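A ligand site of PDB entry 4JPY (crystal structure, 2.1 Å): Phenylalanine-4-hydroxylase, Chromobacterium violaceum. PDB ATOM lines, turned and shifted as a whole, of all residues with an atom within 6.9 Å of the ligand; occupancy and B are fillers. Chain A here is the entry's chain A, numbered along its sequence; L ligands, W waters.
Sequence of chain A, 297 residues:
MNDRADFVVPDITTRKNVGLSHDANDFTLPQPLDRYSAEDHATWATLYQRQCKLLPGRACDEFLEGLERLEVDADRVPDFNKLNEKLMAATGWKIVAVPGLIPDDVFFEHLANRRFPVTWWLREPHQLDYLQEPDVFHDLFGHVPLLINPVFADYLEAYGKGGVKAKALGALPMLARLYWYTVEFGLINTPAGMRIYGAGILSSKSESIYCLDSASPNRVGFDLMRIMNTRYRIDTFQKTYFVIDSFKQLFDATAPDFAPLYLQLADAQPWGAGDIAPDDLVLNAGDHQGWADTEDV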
ATOM      1  N   ASP A 154      13.415  -2.914 -15.423  1.00  0.00           N
ATOM      2  CA  ASP A 154      13.163  -1.454 -15.291  1.00  0.00           C
ATOM      3  C   ASP A 154      11.816  -1.060 -15.921  1.00  0.00           C
ATOM      4  O   ASP A 154      11.110  -0.180 -15.412  1.00  0.00           O
ATOM      5  CB  ASP A 154      14.272  -0.622 -15.952  1.00  0.00           C
ATOM      6  CG  ASP A 154      15.493  -0.429 -15.059  1.00  0.00           C
ATOM      7  OD1 ASP A 154      15.426  -0.708 -13.835  1.00  0.00           O
ATOM      8  OD2 ASP A 154      16.540   0.032 -15.592  1.00  0.00           O
ATOM      9  N   TYR A 155      11.511  -1.692 -17.051  1.00  0.00           N
ATOM     10  CA  TYR A 155      10.220  -1.530 -17.731  1.00  0.00           C
ATOM     11  C   TYR A 155       9.047  -1.840 -16.813  1.00  0.00           C
ATOM     12  O   TYR A 155       8.066  -1.113 -16.775  1.00  0.00           O
ATOM     13  CB  TYR A 155      10.171  -2.395 -18.990  1.00  0.00           C
ATOM     14  CG  TYR A 155       8.790  -2.507 -19.618  1.00  0.00           C
ATOM     15  CD1 TYR A 155       8.170  -1.386 -20.194  1.00  0.00           C
ATOM     16  CD2 TYR A 155       8.102  -3.730 -19.640  1.00  0.00           C
ATOM     17  CE1 TYR A 155       6.922  -1.477 -20.749  1.00  0.00           C
ATOM     18  CE2 TYR A 155       6.829  -3.820 -20.217  1.00  0.00           C
ATOM     19  CZ  TYR A 155       6.241  -2.696 -20.765  1.00  0.00           C
ATOM     20  OH  TYR A 155       5.017  -2.740 -21.370  1.00  0.00           O
ATOM     21  N   LEU A 156       9.154  -2.953 -16.077  1.00  0.00           N
ATOM     22  CA  LEU A 156       8.118  -3.358 -15.140  1.00  0.00           C
ATOM     23  C   LEU A 156       7.964  -2.376 -13.969  1.00  0.00           C
ATOM     24  O   LEU A 156       6.848  -2.013 -13.621  1.00  0.00           O
ATOM     25  CB  LEU A 156       8.406  -4.769 -14.620  1.00  0.00           C
ATOM     26  CG  LEU A 156       7.669  -5.969 -15.235  1.00  0.00           C
ATOM     27  CD1 LEU A 156       7.692  -7.077 -14.185  1.00  0.00           C
ATOM     28  CD2 LEU A 156       6.236  -5.662 -15.660  1.00  0.00           C
ATOM     29  N   GLU A 157       9.076  -1.952 -13.380  1.00  0.00           N
ATOM     30  CA  GLU A 157       9.064  -0.861 -12.405  1.00  0.00           C
ATOM     31  C   GLU A 157       8.383   0.406 -12.966  1.00  0.00           C
ATOM     32  O   GLU A 157       7.501   0.978 -12.318  1.00  0.00           O
ATOM     33  CB  GLU A 157      10.474  -0.524 -11.907  1.00  0.00           C
ATOM     34  CG  GLU A 157      10.459   0.339 -10.646  1.00  0.00           C
ATOM     35  CD  GLU A 157      11.794   0.978 -10.332  1.00  0.00           C
ATOM     36  OE1 GLU A 157      12.809   0.260 -10.213  1.00  0.00           O
ATOM     37  OE2 GLU A 157      11.845   2.205 -10.181  1.00  0.00           O
ATOM     38  N   ALA A 158       8.808   0.851 -14.145  1.00  0.00           N
ATOM     39  CA  ALA A 158       8.222   2.010 -14.834  1.00  0.00           C
ATOM     40  C   ALA A 158       6.704   1.819 -15.019  1.00  0.00           C
ATOM     41  O   ALA A 158       5.900   2.727 -14.748  1.00  0.00           O
ATOM     42  CB  ALA A 158       8.899   2.225 -16.172  1.00  0.00           C
ATOM     43  N   TYR A 159       6.318   0.612 -15.451  1.00  0.00           N
ATOM     44  CA  TYR A 159       4.900   0.254 -15.587  1.00  0.00           C
ATOM     45  C   TYR A 159       4.148   0.438 -14.266  1.00  0.00           C
ATOM     46  O   TYR A 159       3.082   1.075 -14.215  1.00  0.00           O
ATOM     47  CB  TYR A 159       4.721  -1.192 -16.114  1.00  0.00           C
ATOM     48  CG  TYR A 159       3.265  -1.563 -16.192  1.00  0.00           C
ATOM     49  CD1 TYR A 159       2.625  -2.094 -15.074  1.00  0.00           C
ATOM     50  CD2 TYR A 159       2.526  -1.344 -17.359  1.00  0.00           C
ATOM     51  CE1 TYR A 159       1.264  -2.403 -15.097  1.00  0.00           C
ATOM     52  CE2 TYR A 159       1.173  -1.665 -17.399  1.00  0.00           C
ATOM     53  CZ  TYR A 159       0.551  -2.193 -16.254  1.00  0.00           C
ATOM     54  OH  TYR A 159      -0.790  -2.515 -16.274  1.00  0.00           O
ATOM     55  N   GLY A 160       4.688  -0.142 -13.190  1.00  0.00           N
ATOM     56  CA  GLY A 160       4.120   0.001 -11.868  1.00  0.00           C
ATOM     57  C   GLY A 160       3.848   1.458 -11.522  1.00  0.00           C
ATOM     58  O   GLY A 160       2.726   1.817 -11.181  1.00  0.00           O
ATOM     59  N   LYS A 161       4.877   2.284 -11.628  1.00  0.00           N
ATOM     60  CA  LYS A 161       4.789   3.751 -11.400  1.00  0.00           C
ATOM     61  C   LYS A 161       3.781   4.437 -12.295  1.00  0.00           C
ATOM     62  O   LYS A 161       3.103   5.372 -11.859  1.00  0.00           O
ATOM     63  CB  LYS A 161       6.169   4.382 -11.599  1.00  0.00           C
ATOM     64  CG  LYS A 161       7.154   3.884 -10.555  1.00  0.00           C
ATOM     65  CD  LYS A 161       8.488   4.593 -10.623  1.00  0.00           C
ATOM     66  CE  LYS A 161       9.179   4.440  -9.271  1.00  0.00           C
ATOM     67  NZ  LYS A 161      10.599   4.044  -9.466  1.00  0.00           N
ATOM     68  N   GLY A 162       3.675   3.983 -13.551  1.00  0.00           N
ATOM     69  CA  GLY A 162       2.712   4.526 -14.493  1.00  0.00           C
ATOM     70  C   GLY A 162       1.270   4.341 -14.024  1.00  0.00           C
ATOM     71  O   GLY A 162       0.361   4.972 -14.562  1.00  0.00           O
ATOM     72  N   GLY A 163       1.066   3.495 -13.022  1.00  0.00           N
ATOM     73  CA  GLY A 163      -0.294   3.222 -12.502  1.00  0.00           C
ATOM     74  C   GLY A 163      -1.029   4.455 -11.995  1.00  0.00           C
ATOM     75  O   GLY A 163      -2.223   4.617 -12.244  1.00  0.00           O
ATOM     76  N   LYS A 165      -0.684   7.790 -12.708  1.00  0.00           N
ATOM     77  CA  LYS A 165      -1.137   8.724 -13.744  1.00  0.00           C
ATOM     78  C   LYS A 165      -2.383   8.167 -14.474  1.00  0.00           C
ATOM     79  O   LYS A 165      -3.354   8.914 -14.680  1.00  0.00           O
ATOM     80  CB  LYS A 165      -0.016   9.079 -14.730  1.00  0.00           C
ATOM     81  CG  LYS A 165      -0.450   9.960 -15.903  1.00  0.00           C
ATOM     82  CD  LYS A 165       0.612  10.033 -16.995  1.00  0.00           C
ATOM     83  CE  LYS A 165       1.773  10.914 -16.557  1.00  0.00           C
ATOM     84  NZ  LYS A 165       2.936  10.779 -17.470  1.00  0.00           N
ATOM     85  N   ALA A 166      -2.346   6.883 -14.837  1.00  0.00           N
ATOM     86  CA  ALA A 166      -3.448   6.236 -15.542  1.00  0.00           C
ATOM     87  C   ALA A 166      -4.715   6.248 -14.682  1.00  0.00           C
ATOM     88  O   ALA A 166      -5.814   6.462 -15.199  1.00  0.00           O
ATOM     89  CB  ALA A 166      -3.075   4.803 -15.937  1.00  0.00           C
ATOM     90  N   LEU A 175      -3.606   1.396 -19.980  1.00  0.00           N
ATOM     91  CA  LEU A 175      -2.392   0.831 -19.407  1.00  0.00           C
ATOM     92  C   LEU A 175      -2.406  -0.704 -19.322  1.00  0.00           C
ATOM     93  O   LEU A 175      -1.380  -1.356 -19.624  1.00  0.00           O
ATOM     94  CB  LEU A 175      -2.138   1.441 -18.010  1.00  0.00           C
ATOM     95  CG  LEU A 175      -0.738   1.274 -17.384  1.00  0.00           C
ATOM     96  CD1 LEU A 175       0.332   1.663 -18.402  1.00  0.00           C
ATOM     97  CD2 LEU A 175      -0.573   2.090 -16.099  1.00  0.00           C
ATOM     98  N   LEU A 178      -1.661  -2.370 -22.634  1.00  0.00           N
ATOM     99  CA  LEU A 178      -0.214  -2.315 -22.853  1.00  0.00           C
ATOM    100  C   LEU A 178       0.499  -3.470 -22.150  1.00  0.00           C
ATOM    101  O   LEU A 178       1.323  -4.149 -22.769  1.00  0.00           O
ATOM    102  CB  LEU A 178       0.330  -0.959 -22.389  1.00  0.00           C
ATOM    103  CG  LEU A 178       1.870  -0.891 -22.419  1.00  0.00           C
ATOM    104  CD1 LEU A 178       2.328  -0.907 -23.879  1.00  0.00           C
ATOM    105  CD2 LEU A 178       2.383   0.349 -21.694  1.00  0.00           C
ATOM    106  N   LEU A 224       2.662   1.914 -29.472  1.00  0.00           N
ATOM    107  CA  LEU A 224       2.112   2.240 -28.170  1.00  0.00           C
ATOM    108  C   LEU A 224       0.606   2.575 -28.215  1.00  0.00           C
ATOM    109  O   LEU A 224      -0.214   1.944 -27.526  1.00  0.00           O
ATOM    110  CB  LEU A 224       2.933   3.371 -27.563  1.00  0.00           C
ATOM    111  CG  LEU A 224       2.486   3.948 -26.222  1.00  0.00           C
ATOM    112  CD1 LEU A 224       2.292   2.874 -25.154  1.00  0.00           C
ATOM    113  CD2 LEU A 224       3.514   5.005 -25.809  1.00  0.00           C
ATOM    114  N   LEU A 250      11.260  -1.353 -26.306  1.00  0.00           N
ATOM    115  CA  LEU A 250      10.024  -1.364 -25.505  1.00  0.00           C
ATOM    116  C   LEU A 250      10.114  -0.340 -24.378  1.00  0.00           C
ATOM    117  O   LEU A 250       9.153   0.403 -24.145  1.00  0.00           O
ATOM    118  CB  LEU A 250       9.672  -2.769 -24.973  1.00  0.00           C
ATOM    119  CG  LEU A 250       8.525  -2.935 -23.956  1.00  0.00           C
ATOM    120  CD1 LEU A 250       7.231  -2.324 -24.466  1.00  0.00           C
ATOM    121  CD2 LEU A 250       8.298  -4.398 -23.596  1.00  0.00           C
ATOM    122  N   PHE A 251      11.244  -0.310 -23.676  1.00  0.00           N
ATOM    123  CA  PHE A 251      11.464   0.662 -22.610  1.00  0.00           C
ATOM    124  C   PHE A 251      11.460   2.090 -23.151  1.00  0.00           C
ATOM    125  O   PHE A 251      10.856   2.977 -22.562  1.00  0.00           O
ATOM    126  CB  PHE A 251      12.795   0.414 -21.887  1.00  0.00           C
ATOM    127  CG  PHE A 251      13.040   1.347 -20.716  1.00  0.00           C
ATOM    128  CD1 PHE A 251      13.669   2.580 -20.913  1.00  0.00           C
ATOM    129  CD2 PHE A 251      12.638   0.989 -19.430  1.00  0.00           C
ATOM    130  CE1 PHE A 251      13.893   3.451 -19.849  1.00  0.00           C
ATOM    131  CE2 PHE A 251      12.867   1.855 -18.354  1.00  0.00           C
ATOM    132  CZ  PHE A 251      13.491   3.076 -18.569  1.00  0.00           C
ATOM    133  N   ALA A 253      10.122   3.267 -26.069  1.00  0.00           N
ATOM    134  CA  ALA A 253       8.821   3.633 -26.591  1.00  0.00           C
ATOM    135  C   ALA A 253       7.820   3.921 -25.487  1.00  0.00           C
ATOM    136  O   ALA A 253       6.851   4.642 -25.710  1.00  0.00           O
ATOM    137  CB  ALA A 253       8.286   2.545 -27.505  1.00  0.00           C
ATOM    138  N   THR A 254       8.043   3.355 -24.303  1.00  0.00           N
ATOM    139  CA  THR A 254       7.122   3.583 -23.179  1.00  0.00           C
ATOM    140  C   THR A 254       7.625   4.625 -22.163  1.00  0.00           C
ATOM    141  O   THR A 254       7.023   4.826 -21.111  1.00  0.00           O
ATOM    142  CB  THR A 254       6.742   2.243 -22.495  1.00  0.00           C
ATOM    143  OG1 THR A 254       7.944   1.535 -22.154  1.00  0.00           O
ATOM    144  CG2 THR A 254       5.889   1.364 -23.429  1.00  0.00           C
ATOM    145  N   ALA A 255       8.732   5.292 -22.487  1.00  0.00           N
ATOM    146  CA  ALA A 255       9.250   6.379 -21.646  1.00  0.00           C
ATOM    147  C   ALA A 255       8.543   7.758 -21.787  1.00  0.00           C
ATOM    148  O   ALA A 255       8.477   8.499 -20.823  1.00  0.00           O
ATOM    149  CB  ALA A 255      10.771   6.526 -21.810  1.00  0.00           C
ATOM    150  N   PRO A 256       8.015   8.123 -22.984  1.00  0.00           N
ATOM    151  CA  PRO A 256       7.319   9.425 -23.075  1.00  0.00           C
ATOM    152  C   PRO A 256       6.068   9.559 -22.198  1.00  0.00           C
ATOM    153  O   PRO A 256       5.464   8.533 -21.833  1.00  0.00           O
ATOM    154  CB  PRO A 256       6.909   9.494 -24.549  1.00  0.00           C
ATOM    155  CG  PRO A 256       7.959   8.669 -25.234  1.00  0.00           C
ATOM    156  CD  PRO A 256       8.127   7.487 -24.306  1.00  0.00           C
ATOM    157  N   ASP A 257       5.694  10.807 -21.886  1.00  0.00           N
ATOM    158  CA  ASP A 257       4.443  11.154 -21.179  1.00  0.00           C
ATOM    159  C   ASP A 257       3.219  10.523 -21.885  1.00  0.00           C
ATOM    160  O   ASP A 257       2.921  10.835 -23.057  1.00  0.00           O
ATOM    161  CB  ASP A 257       4.320  12.693 -21.081  1.00  0.00           C
ATOM    162  CG  ASP A 257       3.038  13.168 -20.376  1.00  0.00           C
ATOM    163  OD1 ASP A 257       2.281  12.345 -19.765  1.00  0.00           O
ATOM    164  OD2 ASP A 257       2.784  14.400 -20.419  1.00  0.00           O
ATOM    165  N   PHE A 258       2.514   9.635 -21.165  1.00  0.00           N
ATOM    166  CA  PHE A 258       1.317   8.975 -21.686  1.00  0.00           C
ATOM    167  C   PHE A 258       0.053   9.849 -21.591  1.00  0.00           C
ATOM    168  O   PHE A 258      -0.990   9.489 -22.148  1.00  0.00           O
ATOM    169  CB  PHE A 258       1.039   7.657 -20.917  1.00  0.00           C
ATOM    170  CG  PHE A 258       1.874   6.482 -21.357  1.00  0.00           C
ATOM    171  CD1 PHE A 258       3.042   6.648 -22.097  1.00  0.00           C
ATOM    172  CD2 PHE A 258       1.500   5.193 -20.978  1.00  0.00           C
ATOM    173  CE1 PHE A 258       3.806   5.563 -22.481  1.00  0.00           C
ATOM    174  CE2 PHE A 258       2.261   4.084 -21.344  1.00  0.00           C
ATOM    175  CZ  PHE A 258       3.419   4.275 -22.104  1.00  0.00           C
ATOM    176  N   ALA A 259       0.142  10.980 -20.882  1.00  0.00           N
ATOM    177  CA  ALA A 259      -1.076  11.790 -20.644  1.00  0.00           C
ATOM    178  C   ALA A 259      -1.810  12.224 -21.927  1.00  0.00           C
ATOM    179  O   ALA A 259      -3.014  12.030 -22.017  1.00  0.00           O
ATOM    180  CB  ALA A 259      -0.796  12.987 -19.720  1.00  0.00           C
ATOM    181  N   TYR A 262      -3.504   9.135 -23.513  1.00  0.00           N
ATOM    182  CA  TYR A 262      -4.709   8.733 -22.779  1.00  0.00           C
ATOM    183  C   TYR A 262      -5.915   9.593 -23.101  1.00  0.00           C
ATOM    184  O   TYR A 262      -7.027   9.104 -23.250  1.00  0.00           O
ATOM    185  CB  TYR A 262      -4.494   8.799 -21.262  1.00  0.00           C
ATOM    186  CG  TYR A 262      -3.547   7.796 -20.643  1.00  0.00           C
ATOM    187  CD1 TYR A 262      -3.403   6.497 -21.142  1.00  0.00           C
ATOM    188  CD2 TYR A 262      -2.832   8.146 -19.506  1.00  0.00           C
ATOM    189  CE1 TYR A 262      -2.546   5.584 -20.522  1.00  0.00           C
ATOM    190  CE2 TYR A 262      -1.989   7.249 -18.883  1.00  0.00           C
ATOM    191  CZ  TYR A 262      -1.849   5.979 -19.395  1.00  0.00           C
ATOM    192  OH  TYR A 262      -0.987   5.119 -18.752  1.00  0.00           O
HETATM  193  N1  LIG L   1       5.691   6.729 -19.610  1.00  0.00           N
HETATM  194  C1  LIG L   1       4.475   6.307 -18.854  1.00  0.00           C
HETATM  195  C2  LIG L   1       3.717   7.522 -18.344  1.00  0.00           C
HETATM  196  O1  LIG L   1       2.811   7.420 -17.530  1.00  0.00           O
HETATM  197  C3  LIG L   1       4.845   5.343 -17.706  1.00  0.00           C
HETATM  198  C4  LIG L   1       4.960   3.891 -18.147  1.00  0.00           C
HETATM  199  C5  LIG L   1       3.803   3.094 -18.265  1.00  0.00           C
HETATM  200  C6  LIG L   1       6.179   3.344 -18.468  1.00  0.00           C
HETATM  201  C7  LIG L   1       3.897   1.761 -18.683  1.00  0.00           C
HETATM  202  C8  LIG L   1       6.272   2.004 -18.880  1.00  0.00           C
HETATM  203  C9  LIG L   1       5.141   1.214 -18.983  1.00  0.00           C
HETATM  204  O2  LIG L   1       3.990   8.642 -18.769  1.00  0.00           O
HETATM  205  O   HOH W   1       0.610   6.013 -16.942  1.00  0.00           O
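N1 of the ligand is in hydrogen-bond range of O of Pro 256, at 2.9 Å. An oxygen (O2) of the ligand is in hydrogen-bond range of the backbone NH (N) of Phe 258 (3.0 Å). The side-chain amino group (NZ) of Lys 165 lies within salt-bridge range of an oxygen (O2) of the ligand. A nitrogen (N1) of the ligand sits at hydrogen-bond distance from the backbone carbonyl oxygen (O) of Thr 254 (2.8 Å).
NZ of Lys 165 lies within salt-bridge range of OD1 of Asp 257, 2.9 Å away. The side-chain hydroxyl of Thr 254 lies within hydrogen-bond range of the backbone carbonyl oxygen of Phe 251 (3.3 Å). The backbone carbonyl oxygen (O) of Leu 250 sits at hydrogen-bond distance from the side-chain hydroxyl (OG1) of Thr 254, at 2.6 Å. OD1 of Asp 257 is in hydrogen-bond range of N of Ala 259 (2.8 Å).
Merely in contact with the ligand: Tyr 155 (3.7 Å), Ala 158 (3.7 Å), Tyr 159 (3.5 Å), Gly 162 (3.9 Å), Leu 175 (3.6 Å), Leu 178 (3.7 Å), Ala 255 (3.5 Å) and Asp 257 (3.5 Å). Hydrophobic or aromatic side chains that line the ligand: Tyr 155, Ala 158, Tyr 159, Leu 175, Leu 178 and Phe 258. Of the 25 residues printed, 12 come within 4 Å of the ligand. The nearest printed residue that does not touch the ligand is Tyr 262 (4.6 Å).
Water W1 lies within hydrogen-bond range of OH of Tyr 262, O of Gly 162 and O1 of the ligand.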
